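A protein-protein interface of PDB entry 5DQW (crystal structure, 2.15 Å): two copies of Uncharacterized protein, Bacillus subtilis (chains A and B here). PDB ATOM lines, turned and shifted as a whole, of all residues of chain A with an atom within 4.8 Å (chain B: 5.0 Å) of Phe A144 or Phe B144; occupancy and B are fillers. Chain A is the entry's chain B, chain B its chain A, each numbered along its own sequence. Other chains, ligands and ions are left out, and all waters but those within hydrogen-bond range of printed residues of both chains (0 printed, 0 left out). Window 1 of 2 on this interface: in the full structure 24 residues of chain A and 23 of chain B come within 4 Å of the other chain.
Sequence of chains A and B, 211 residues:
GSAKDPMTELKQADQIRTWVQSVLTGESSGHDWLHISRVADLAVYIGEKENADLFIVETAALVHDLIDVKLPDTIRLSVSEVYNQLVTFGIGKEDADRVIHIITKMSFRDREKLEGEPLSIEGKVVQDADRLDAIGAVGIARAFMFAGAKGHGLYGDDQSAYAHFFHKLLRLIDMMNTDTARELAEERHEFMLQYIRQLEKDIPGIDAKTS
Among the printed residues, pairs that only touch across the chains: Ala A141 with Phe B144 (3.6 Å), Ala A141 with Leu B154 (3.9 Å), Ala A141 with Tyr B195 (3.4 Å), Arg A142 with Leu B154 (3.9 Å), Phe A144 with Ala B141 (3.6 Å), Phe A144 with Phe B144 (3.9 Å), Phe A144 with Met B145 (3.4 Å), Met A145 with Phe B144 (3.4 Å), Met A145 with Gly B148 (3.3 Å), Met A145 with Leu B154 (3.7 Å), Gly A148 with Met B145 (3.4 Å), Gly A148 with Gly B148 (3.9 Å), Gly A148 with Ala B149 (3.7 Å), Leu A154 with Ala B141 (3.9 Å), Leu A154 with Met B145 (3.5 Å) and Tyr A195 with Ala B141 (3.4 Å).
Of the 15 printed residues of chain A, 7 touch a printed residue of chain B.
Printed residues of chain B that touch a printed residue of chain A: Ala B141, Phe B144, Met B145, Gly B148, Ala B149, Leu B154 and Tyr B195.
Hydrophobic or aromatic side chains of chain B within 4 Å of the printed part of chain A: Ala B141, Phe B144, Met B145, Ala B149, Leu B154 and Tyr B195.
The backbone carbonyl oxygen of Leu B154 sits at hydrogen-bond distance from the backbone NH of Tyr B162 (2.9 Å).
O of Leu A154 sits at hydrogen-bond distance from N of Tyr A162, 3.0 Å away.
Ala A141 touches Phe B144, and with the chains exchanged Phe A144 touches Ala B141.
Ala A141 touches Leu B154, and with the chains exchanged Leu A154 touches Ala B141.
Ala A141 touches Tyr B195, and with the chains exchanged Tyr A195 touches Ala B141.
Phe B144 touches its own counterpart, Phe A144.
Positions printed for both chains: 140, 141, 142, 143, 144, 145, 146, 147, 148, 154, 161, 162, 165, 195 and 199.
Of the 16 pairs that touch across the chains among the printed residues, 14 have their exchanged pair printed and touching as well.
Phe B144 touches just these residues of chain A: Ala A141, Phe A144 and Met A145.
Of the printed residues of chain A, Ala B149 touches Gly A148.
Of the printed residues of chain A, Ala B141 touches Phe A144 (3.6 Å), Leu A154 (3.9 Å) and Tyr A195 (3.4 Å).
Phe B146 touches none of the printed residues of chain A.
Leu B199 touches none of the printed residues of chain A.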
ATOM      1  N   ILE A 140     -24.956  21.755   7.430  1.00  0.00           N
ATOM      2  CA  ILE A 140     -24.410  21.320   6.172  1.00  0.00           C
ATOM      3  C   ILE A 140     -23.127  22.112   5.938  1.00  0.00           C
ATOM      4  O   ILE A 140     -22.072  21.552   5.630  1.00  0.00           O
ATOM      5  CB  ILE A 140     -25.455  21.528   5.032  1.00  0.00           C
ATOM      6  CG1 ILE A 140     -26.566  20.478   5.155  1.00  0.00           C
ATOM      7  CG2 ILE A 140     -24.792  21.538   3.653  1.00  0.00           C
ATOM      8  CD1 ILE A 140     -27.918  20.808   4.403  1.00  0.00           C
ATOM      9  N   ALA A 141     -23.227  23.422   6.098  1.00  0.00           N
ATOM     10  CA  ALA A 141     -22.104  24.299   5.851  1.00  0.00           C
ATOM     11  C   ALA A 141     -20.911  23.906   6.697  1.00  0.00           C
ATOM     12  O   ALA A 141     -19.816  23.763   6.176  1.00  0.00           O
ATOM     13  CB  ALA A 141     -22.482  25.777   6.105  1.00  0.00           C
ATOM     14  N   ARG A 142     -21.131  23.697   7.989  1.00  0.00           N
ATOM     15  CA  ARG A 142     -20.029  23.433   8.913  1.00  0.00           C
ATOM     16  C   ARG A 142     -19.414  22.070   8.640  1.00  0.00           C
ATOM     17  O   ARG A 142     -18.211  21.881   8.825  1.00  0.00           O
ATOM     18  CB  ARG A 142     -20.514  23.529  10.359  1.00  0.00           C
ATOM     19  CG  ARG A 142     -21.048  24.928  10.791  1.00  0.00           C
ATOM     20  CD  ARG A 142     -21.770  24.804  12.150  1.00  0.00           C
ATOM     21  NE  ARG A 142     -20.780  24.524  13.184  1.00  0.00           N
ATOM     22  CZ  ARG A 142     -20.980  23.805  14.288  1.00  0.00           C
ATOM     23  NH1 ARG A 142     -22.177  23.265  14.566  1.00  0.00           N
ATOM     24  NH2 ARG A 142     -19.958  23.615  15.121  1.00  0.00           N
ATOM     25  N   ALA A 143     -20.232  21.123   8.173  1.00  0.00           N
ATOM     26  CA  ALA A 143     -19.758  19.786   7.915  1.00  0.00           C
ATOM     27  C   ALA A 143     -18.802  19.843   6.754  1.00  0.00           C
ATOM     28  O   ALA A 143     -17.734  19.263   6.793  1.00  0.00           O
ATOM     29  CB  ALA A 143     -20.923  18.820   7.598  1.00  0.00           C
ATOM     30  N   PHE A 144     -19.205  20.525   5.689  1.00  0.00           N
ATOM     31  CA  PHE A 144     -18.298  20.692   4.566  1.00  0.00           C
ATOM     32  C   PHE A 144     -17.074  21.577   4.882  1.00  0.00           C
ATOM     33  O   PHE A 144     -15.964  21.253   4.440  1.00  0.00           O
ATOM     34  CB  PHE A 144     -19.077  21.141   3.351  1.00  0.00           C
ATOM     35  CG  PHE A 144     -19.956  20.050   2.776  1.00  0.00           C
ATOM     36  CD1 PHE A 144     -19.387  18.914   2.225  1.00  0.00           C
ATOM     37  CD2 PHE A 144     -21.315  20.182   2.732  1.00  0.00           C
ATOM     38  CE1 PHE A 144     -20.168  17.918   1.663  1.00  0.00           C
ATOM     39  CE2 PHE A 144     -22.114  19.157   2.173  1.00  0.00           C
ATOM     40  CZ  PHE A 144     -21.517  18.023   1.659  1.00  0.00           C
ATOM     41  N   MET A 145     -17.241  22.651   5.663  1.00  0.00           N
ATOM     42  CA  MET A 145     -16.075  23.429   6.136  1.00  0.00           C
ATOM     43  C   MET A 145     -15.104  22.566   6.901  1.00  0.00           C
ATOM     44  O   MET A 145     -13.891  22.654   6.689  1.00  0.00           O
ATOM     45  CB  MET A 145     -16.494  24.621   7.017  1.00  0.00           C
ATOM     46  CG  MET A 145     -17.177  25.693   6.177  1.00  0.00           C
ATOM     47  SD  MET A 145     -17.603  27.227   6.995  1.00  0.00           S
ATOM     48  CE  MET A 145     -16.024  28.034   7.152  1.00  0.00           C
ATOM     49  N   PHE A 146     -15.641  21.731   7.792  1.00  0.00           N
ATOM     50  CA  PHE A 146     -14.855  20.760   8.551  1.00  0.00           C
ATOM     51  C   PHE A 146     -14.104  19.828   7.599  1.00  0.00           C
ATOM     52  O   PHE A 146     -12.886  19.619   7.749  1.00  0.00           O
ATOM     53  CB  PHE A 146     -15.768  19.937   9.467  1.00  0.00           C
ATOM     54  CG  PHE A 146     -15.035  19.033  10.457  1.00  0.00           C
ATOM     55  CD1 PHE A 146     -14.675  19.507  11.703  1.00  0.00           C
ATOM     56  CD2 PHE A 146     -14.759  17.715  10.150  1.00  0.00           C
ATOM     57  CE1 PHE A 146     -14.026  18.679  12.641  1.00  0.00           C
ATOM     58  CE2 PHE A 146     -14.112  16.871  11.082  1.00  0.00           C
ATOM     59  CZ  PHE A 146     -13.735  17.365  12.317  1.00  0.00           C
ATOM     60  N   ALA A 147     -14.815  19.250   6.626  1.00  0.00           N
ATOM     61  CA  ALA A 147     -14.161  18.287   5.721  1.00  0.00           C
ATOM     62  C   ALA A 147     -13.047  18.959   4.924  1.00  0.00           C
ATOM     63  O   ALA A 147     -11.985  18.358   4.658  1.00  0.00           O
ATOM     64  CB  ALA A 147     -15.155  17.648   4.788  1.00  0.00           C
ATOM     65  N   GLY A 148     -13.288  20.202   4.537  1.00  0.00           N
ATOM     66  CA  GLY A 148     -12.281  20.987   3.836  1.00  0.00           C
ATOM     67  C   GLY A 148     -11.082  21.312   4.701  1.00  0.00           C
ATOM     68  O   GLY A 148      -9.955  21.219   4.242  1.00  0.00           O
ATOM     69  N   LEU A 154     -15.415  15.154  -0.135  1.00  0.00           N
ATOM     70  CA  LEU A 154     -16.836  15.465  -0.162  1.00  0.00           C
ATOM     71  C   LEU A 154     -17.608  14.170   0.125  1.00  0.00           C
ATOM     72  O   LEU A 154     -18.527  14.161   0.962  1.00  0.00           O
ATOM     73  CB  LEU A 154     -17.228  16.057  -1.529  1.00  0.00           C
ATOM     74  CG  LEU A 154     -18.518  16.849  -1.750  1.00  0.00           C
ATOM     75  CD1 LEU A 154     -18.468  17.589  -3.118  1.00  0.00           C
ATOM     76  CD2 LEU A 154     -19.730  15.936  -1.681  1.00  0.00           C
ATOM     77  N   ALA A 161     -17.429  14.030   4.324  1.00  0.00           N
ATOM     78  CA  ALA A 161     -18.552  14.850   4.831  1.00  0.00           C
ATOM     79  C   ALA A 161     -19.870  14.098   4.651  1.00  0.00           C
ATOM     80  O   ALA A 161     -20.678  14.002   5.584  1.00  0.00           O
ATOM     81  CB  ALA A 161     -18.605  16.201   4.124  1.00  0.00           C
ATOM     82  N   TYR A 162     -20.073  13.550   3.457  1.00  0.00           N
ATOM     83  CA  TYR A 162     -21.329  12.895   3.116  1.00  0.00           C
ATOM     84  C   TYR A 162     -21.615  11.734   4.079  1.00  0.00           C
ATOM     85  O   TYR A 162     -22.730  11.559   4.554  1.00  0.00           O
ATOM     86  CB  TYR A 162     -21.248  12.417   1.674  1.00  0.00           C
ATOM     87  CG  TYR A 162     -22.483  11.747   1.166  1.00  0.00           C
ATOM     88  CD1 TYR A 162     -23.691  12.450   1.077  1.00  0.00           C
ATOM     89  CD2 TYR A 162     -22.456  10.421   0.745  1.00  0.00           C
ATOM     90  CE1 TYR A 162     -24.842  11.823   0.606  1.00  0.00           C
ATOM     91  CE2 TYR A 162     -23.613   9.788   0.273  1.00  0.00           C
ATOM     92  CZ  TYR A 162     -24.789  10.523   0.195  1.00  0.00           C
ATOM     93  OH  TYR A 162     -25.933   9.929  -0.266  1.00  0.00           O
ATOM     94  N   PHE A 165     -23.209  12.759   7.557  1.00  0.00           N
ATOM     95  CA  PHE A 165     -24.662  12.890   7.612  1.00  0.00           C
ATOM     96  C   PHE A 165     -25.359  11.662   8.206  1.00  0.00           C
ATOM     97  O   PHE A 165     -26.171  11.792   9.126  1.00  0.00           O
ATOM     98  CB  PHE A 165     -25.197  13.205   6.222  1.00  0.00           C
ATOM     99  CG  PHE A 165     -24.959  14.615   5.821  1.00  0.00           C
ATOM    100  CD1 PHE A 165     -25.826  15.623   6.242  1.00  0.00           C
ATOM    101  CD2 PHE A 165     -23.856  14.954   5.080  1.00  0.00           C
ATOM    102  CE1 PHE A 165     -25.586  16.954   5.892  1.00  0.00           C
ATOM    103  CE2 PHE A 165     -23.602  16.285   4.723  1.00  0.00           C
ATOM    104  CZ  PHE A 165     -24.470  17.278   5.124  1.00  0.00           C
ATOM    105  N   TYR A 195     -31.525  18.540   0.864  1.00  0.00           N
ATOM    106  CA  TYR A 195     -30.124  18.739   0.445  1.00  0.00           C
ATOM    107  C   TYR A 195     -29.490  17.451  -0.060  1.00  0.00           C
ATOM    108  O   TYR A 195     -28.948  17.390  -1.185  1.00  0.00           O
ATOM    109  CB  TYR A 195     -29.267  19.365   1.586  1.00  0.00           C
ATOM    110  CG  TYR A 195     -27.851  19.598   1.128  1.00  0.00           C
ATOM    111  CD1 TYR A 195     -27.513  20.726   0.393  1.00  0.00           C
ATOM    112  CD2 TYR A 195     -26.877  18.640   1.329  1.00  0.00           C
ATOM    113  CE1 TYR A 195     -26.198  20.906  -0.092  1.00  0.00           C
ATOM    114  CE2 TYR A 195     -25.586  18.800   0.837  1.00  0.00           C
ATOM    115  CZ  TYR A 195     -25.255  19.920   0.129  1.00  0.00           C
ATOM    116  OH  TYR A 195     -23.964  20.047  -0.349  1.00  0.00           O
ATOM    117  N   LEU A 199     -28.131  16.408  -3.776  1.00  0.00           N
ATOM    118  CA  LEU A 199     -26.762  15.970  -3.933  1.00  0.00           C
ATOM    119  C   LEU A 199     -26.719  14.642  -4.701  1.00  0.00           C
ATOM    120  O   LEU A 199     -25.873  14.463  -5.570  1.00  0.00           O
ATOM    121  CB  LEU A 199     -26.052  15.890  -2.573  1.00  0.00           C
ATOM    122  CG  LEU A 199     -24.513  15.945  -2.618  1.00  0.00           C
ATOM    123  CD1 LEU A 199     -23.950  17.253  -3.184  1.00  0.00           C
ATOM    124  CD2 LEU A 199     -23.915  15.695  -1.251  1.00  0.00           C
ATOM    125  N   ILE B 140     -22.565  24.100  -3.528  1.00  0.00           N
ATOM    126  CA  ILE B 140     -22.627  24.491  -2.108  1.00  0.00           C
ATOM    127  C   ILE B 140     -21.578  23.757  -1.276  1.00  0.00           C
ATOM    128  O   ILE B 140     -20.864  24.352  -0.473  1.00  0.00           O
ATOM    129  CB  ILE B 140     -24.049  24.219  -1.502  1.00  0.00           C
ATOM    130  CG1 ILE B 140     -25.065  25.234  -2.058  1.00  0.00           C
ATOM    131  CG2 ILE B 140     -24.000  24.314   0.020  1.00  0.00           C
ATOM    132  CD1 ILE B 140     -26.478  24.796  -1.933  1.00  0.00           C
ATOM    133  N   ALA B 141     -21.502  22.459  -1.466  1.00  0.00           N
ATOM    134  CA  ALA B 141     -20.514  21.621  -0.755  1.00  0.00           C
ATOM    135  C   ALA B 141     -19.102  22.079  -1.076  1.00  0.00           C
ATOM    136  O   ALA B 141     -18.308  22.316  -0.188  1.00  0.00           O
ATOM    137  CB  ALA B 141     -20.695  20.135  -1.137  1.00  0.00           C
ATOM    138  N   ARG B 142     -18.838  22.264  -2.367  1.00  0.00           N
ATOM    139  CA  ARG B 142     -17.495  22.653  -2.825  1.00  0.00           C
ATOM    140  C   ARG B 142     -17.109  24.035  -2.292  1.00  0.00           C
ATOM    141  O   ARG B 142     -15.961  24.239  -1.850  1.00  0.00           O
ATOM    142  CB  ARG B 142     -17.379  22.562  -4.351  1.00  0.00           C
ATOM    143  CG  ARG B 142     -17.440  21.136  -4.900  1.00  0.00           C
ATOM    144  CD  ARG B 142     -17.472  21.182  -6.430  1.00  0.00           C
ATOM    145  NE  ARG B 142     -16.142  21.546  -6.905  1.00  0.00           N
ATOM    146  CZ  ARG B 142     -15.848  22.326  -7.932  1.00  0.00           C
ATOM    147  NH1 ARG B 142     -16.780  22.811  -8.732  1.00  0.00           N
ATOM    148  NH2 ARG B 142     -14.579  22.595  -8.173  1.00  0.00           N
ATOM    149  N   ALA B 143     -18.070  24.950  -2.243  1.00  0.00           N
ATOM    150  CA  ALA B 143     -17.826  26.300  -1.699  1.00  0.00           C
ATOM    151  C   ALA B 143     -17.438  26.287  -0.221  1.00  0.00           C
ATOM    152  O   ALA B 143     -16.469  26.947   0.203  1.00  0.00           O
ATOM    153  CB  ALA B 143     -19.062  27.221  -1.910  1.00  0.00           C
ATOM    154  N   PHE B 144     -18.200  25.560   0.587  1.00  0.00           N
ATOM    155  CA  PHE B 144     -17.860  25.469   2.013  1.00  0.00           C
ATOM    156  C   PHE B 144     -16.569  24.655   2.281  1.00  0.00           C
ATOM    157  O   PHE B 144     -15.789  25.003   3.168  1.00  0.00           O
ATOM    158  CB  PHE B 144     -19.067  24.978   2.821  1.00  0.00           C
ATOM    159  CG  PHE B 144     -20.216  26.023   2.911  1.00  0.00           C
ATOM    160  CD1 PHE B 144     -20.063  27.159   3.650  1.00  0.00           C
ATOM    161  CD2 PHE B 144     -21.410  25.827   2.271  1.00  0.00           C
ATOM    162  CE1 PHE B 144     -21.066  28.100   3.732  1.00  0.00           C
ATOM    163  CE2 PHE B 144     -22.432  26.736   2.375  1.00  0.00           C
ATOM    164  CZ  PHE B 144     -22.249  27.884   3.086  1.00  0.00           C
ATOM    165  N   MET B 145     -16.305  23.607   1.505  1.00  0.00           N
ATOM    166  CA  MET B 145     -14.980  22.927   1.596  1.00  0.00           C
ATOM    167  C   MET B 145     -13.804  23.870   1.311  1.00  0.00           C
ATOM    168  O   MET B 145     -12.806  23.849   2.021  1.00  0.00           O
ATOM    169  CB  MET B 145     -14.895  21.709   0.653  1.00  0.00           C
ATOM    170  CG  MET B 145     -15.836  20.537   1.061  1.00  0.00           C
ATOM    171  SD  MET B 145     -15.753  19.002   0.085  1.00  0.00           S
ATOM    172  CE  MET B 145     -14.207  18.319   0.700  1.00  0.00           C
ATOM    173  N   PHE B 146     -13.901  24.650   0.240  1.00  0.00           N
ATOM    174  CA  PHE B 146     -12.907  25.676  -0.094  1.00  0.00           C
ATOM    175  C   PHE B 146     -12.683  26.647   1.072  1.00  0.00           C
ATOM    176  O   PHE B 146     -11.526  26.902   1.490  1.00  0.00           O
ATOM    177  CB  PHE B 146     -13.368  26.426  -1.369  1.00  0.00           C
ATOM    178  CG  PHE B 146     -12.392  27.464  -1.872  1.00  0.00           C
ATOM    179  CD1 PHE B 146     -12.368  28.759  -1.318  1.00  0.00           C
ATOM    180  CD2 PHE B 146     -11.487  27.158  -2.878  1.00  0.00           C
ATOM    181  CE1 PHE B 146     -11.458  29.733  -1.774  1.00  0.00           C
ATOM    182  CE2 PHE B 146     -10.553  28.120  -3.330  1.00  0.00           C
ATOM    183  CZ  PHE B 146     -10.556  29.414  -2.779  1.00  0.00           C
ATOM    184  N   ALA B 147     -13.786  27.186   1.615  1.00  0.00           N
ATOM    185  CA  ALA B 147     -13.713  28.105   2.740  1.00  0.00           C
ATOM    186  C   ALA B 147     -12.983  27.446   3.907  1.00  0.00           C
ATOM    187  O   ALA B 147     -12.104  28.064   4.542  1.00  0.00           O
ATOM    188  CB  ALA B 147     -15.100  28.551   3.159  1.00  0.00           C
ATOM    189  N   GLY B 148     -13.360  26.193   4.190  1.00  0.00           N
ATOM    190  CA  GLY B 148     -12.720  25.415   5.256  1.00  0.00           C
ATOM    191  C   GLY B 148     -11.239  25.233   4.951  1.00  0.00           C
ATOM    192  O   GLY B 148     -10.405  25.402   5.810  1.00  0.00           O
ATOM    193  N   ALA B 149     -10.918  24.935   3.696  1.00  0.00           N
ATOM    194  CA  ALA B 149      -9.519  24.724   3.294  1.00  0.00           C
ATOM    195  C   ALA B 149      -8.659  25.983   3.465  1.00  0.00           C
ATOM    196  O   ALA B 149      -7.486  25.900   3.877  1.00  0.00           O
ATOM    197  CB  ALA B 149      -9.446  24.218   1.855  1.00  0.00           C
ATOM    198  N   LEU B 154     -17.777  31.263   7.434  1.00  0.00           N
ATOM    199  CA  LEU B 154     -18.984  30.767   6.833  1.00  0.00           C
ATOM    200  C   LEU B 154     -19.715  31.967   6.225  1.00  0.00           C
ATOM    201  O   LEU B 154     -20.187  31.927   5.085  1.00  0.00           O
ATOM    202  CB  LEU B 154     -19.813  30.101   7.920  1.00  0.00           C
ATOM    203  CG  LEU B 154     -20.839  29.042   7.538  1.00  0.00           C
ATOM    204  CD1 LEU B 154     -21.200  28.270   8.822  1.00  0.00           C
ATOM    205  CD2 LEU B 154     -22.085  29.642   6.831  1.00  0.00           C
ATOM    206  N   ALA B 161     -17.579  32.292   2.728  1.00  0.00           N
ATOM    207  CA  ALA B 161     -18.258  31.389   1.821  1.00  0.00           C
ATOM    208  C   ALA B 161     -19.585  32.007   1.373  1.00  0.00           C
ATOM    209  O   ALA B 161     -19.951  31.931   0.203  1.00  0.00           O
ATOM    210  CB  ALA B 161     -18.498  30.040   2.484  1.00  0.00           C
ATOM    211  N   TYR B 162     -20.300  32.618   2.310  1.00  0.00           N
ATOM    212  CA  TYR B 162     -21.600  33.265   1.988  1.00  0.00           C
ATOM    213  C   TYR B 162     -21.428  34.409   0.980  1.00  0.00           C
ATOM    214  O   TYR B 162     -22.189  34.495   0.002  1.00  0.00           O
ATOM    215  CB  TYR B 162     -22.268  33.765   3.262  1.00  0.00           C
ATOM    216  CG  TYR B 162     -23.722  34.171   3.142  1.00  0.00           C
ATOM    217  CD1 TYR B 162     -24.696  33.238   2.869  1.00  0.00           C
ATOM    218  CD2 TYR B 162     -24.122  35.488   3.388  1.00  0.00           C
ATOM    219  CE1 TYR B 162     -26.052  33.602   2.787  1.00  0.00           C
ATOM    220  CE2 TYR B 162     -25.462  35.870   3.320  1.00  0.00           C
ATOM    221  CZ  TYR B 162     -26.428  34.916   3.009  1.00  0.00           C
ATOM    222  OH  TYR B 162     -27.750  35.255   2.920  1.00  0.00           O
ATOM    223  N   PHE B 165     -21.212  33.193  -2.604  1.00  0.00           N
ATOM    224  CA  PHE B 165     -22.466  32.906  -3.261  1.00  0.00           C
ATOM    225  C   PHE B 165     -22.910  34.137  -4.018  1.00  0.00           C
ATOM    226  O   PHE B 165     -23.285  34.023  -5.204  1.00  0.00           O
ATOM    227  CB  PHE B 165     -23.551  32.457  -2.284  1.00  0.00           C
ATOM    228  CG  PHE B 165     -23.416  31.017  -1.856  1.00  0.00           C
ATOM    229  CD1 PHE B 165     -22.534  30.668  -0.841  1.00  0.00           C
ATOM    230  CD2 PHE B 165     -24.128  30.023  -2.493  1.00  0.00           C
ATOM    231  CE1 PHE B 165     -22.382  29.342  -0.437  1.00  0.00           C
ATOM    232  CE2 PHE B 165     -23.992  28.684  -2.107  1.00  0.00           C
ATOM    233  CZ  PHE B 165     -23.125  28.344  -1.068  1.00  0.00           C
ATOM    234  N   TYR B 195     -31.357  27.062  -0.510  1.00  0.00           N
ATOM    235  CA  TYR B 195     -30.288  26.896   0.515  1.00  0.00           C
ATOM    236  C   TYR B 195     -30.018  28.219   1.240  1.00  0.00           C
ATOM    237  O   TYR B 195     -29.965  28.275   2.481  1.00  0.00           O
ATOM    238  CB  TYR B 195     -28.999  26.284  -0.093  1.00  0.00           C
ATOM    239  CG  TYR B 195     -27.963  26.119   0.967  1.00  0.00           C
ATOM    240  CD1 TYR B 195     -27.106  27.158   1.256  1.00  0.00           C
ATOM    241  CD2 TYR B 195     -27.867  24.957   1.730  1.00  0.00           C
ATOM    242  CE1 TYR B 195     -26.177  27.064   2.243  1.00  0.00           C
ATOM    243  CE2 TYR B 195     -26.905  24.869   2.743  1.00  0.00           C
ATOM    244  CZ  TYR B 195     -26.081  25.939   2.980  1.00  0.00           C
ATOM    245  OH  TYR B 195     -25.146  25.942   3.970  1.00  0.00           O
ATOM    246  N   LEU B 199     -30.526  29.276   5.154  1.00  0.00           N
ATOM    247  CA  LEU B 199     -29.497  29.877   5.976  1.00  0.00           C
ATOM    248  C   LEU B 199     -30.014  31.168   6.588  1.00  0.00           C
ATOM    249  O   LEU B 199     -29.735  31.453   7.734  1.00  0.00           O
ATOM    250  CB  LEU B 199     -28.241  30.236   5.188  1.00  0.00           C
ATOM    251  CG  LEU B 199     -27.044  29.307   5.098  1.00  0.00           C
ATOM    252  CD1 LEU B 199     -25.897  30.166   4.523  1.00  0.00           C
ATOM    253  CD2 LEU B 199     -26.672  28.632   6.456  1.00  0.00           C
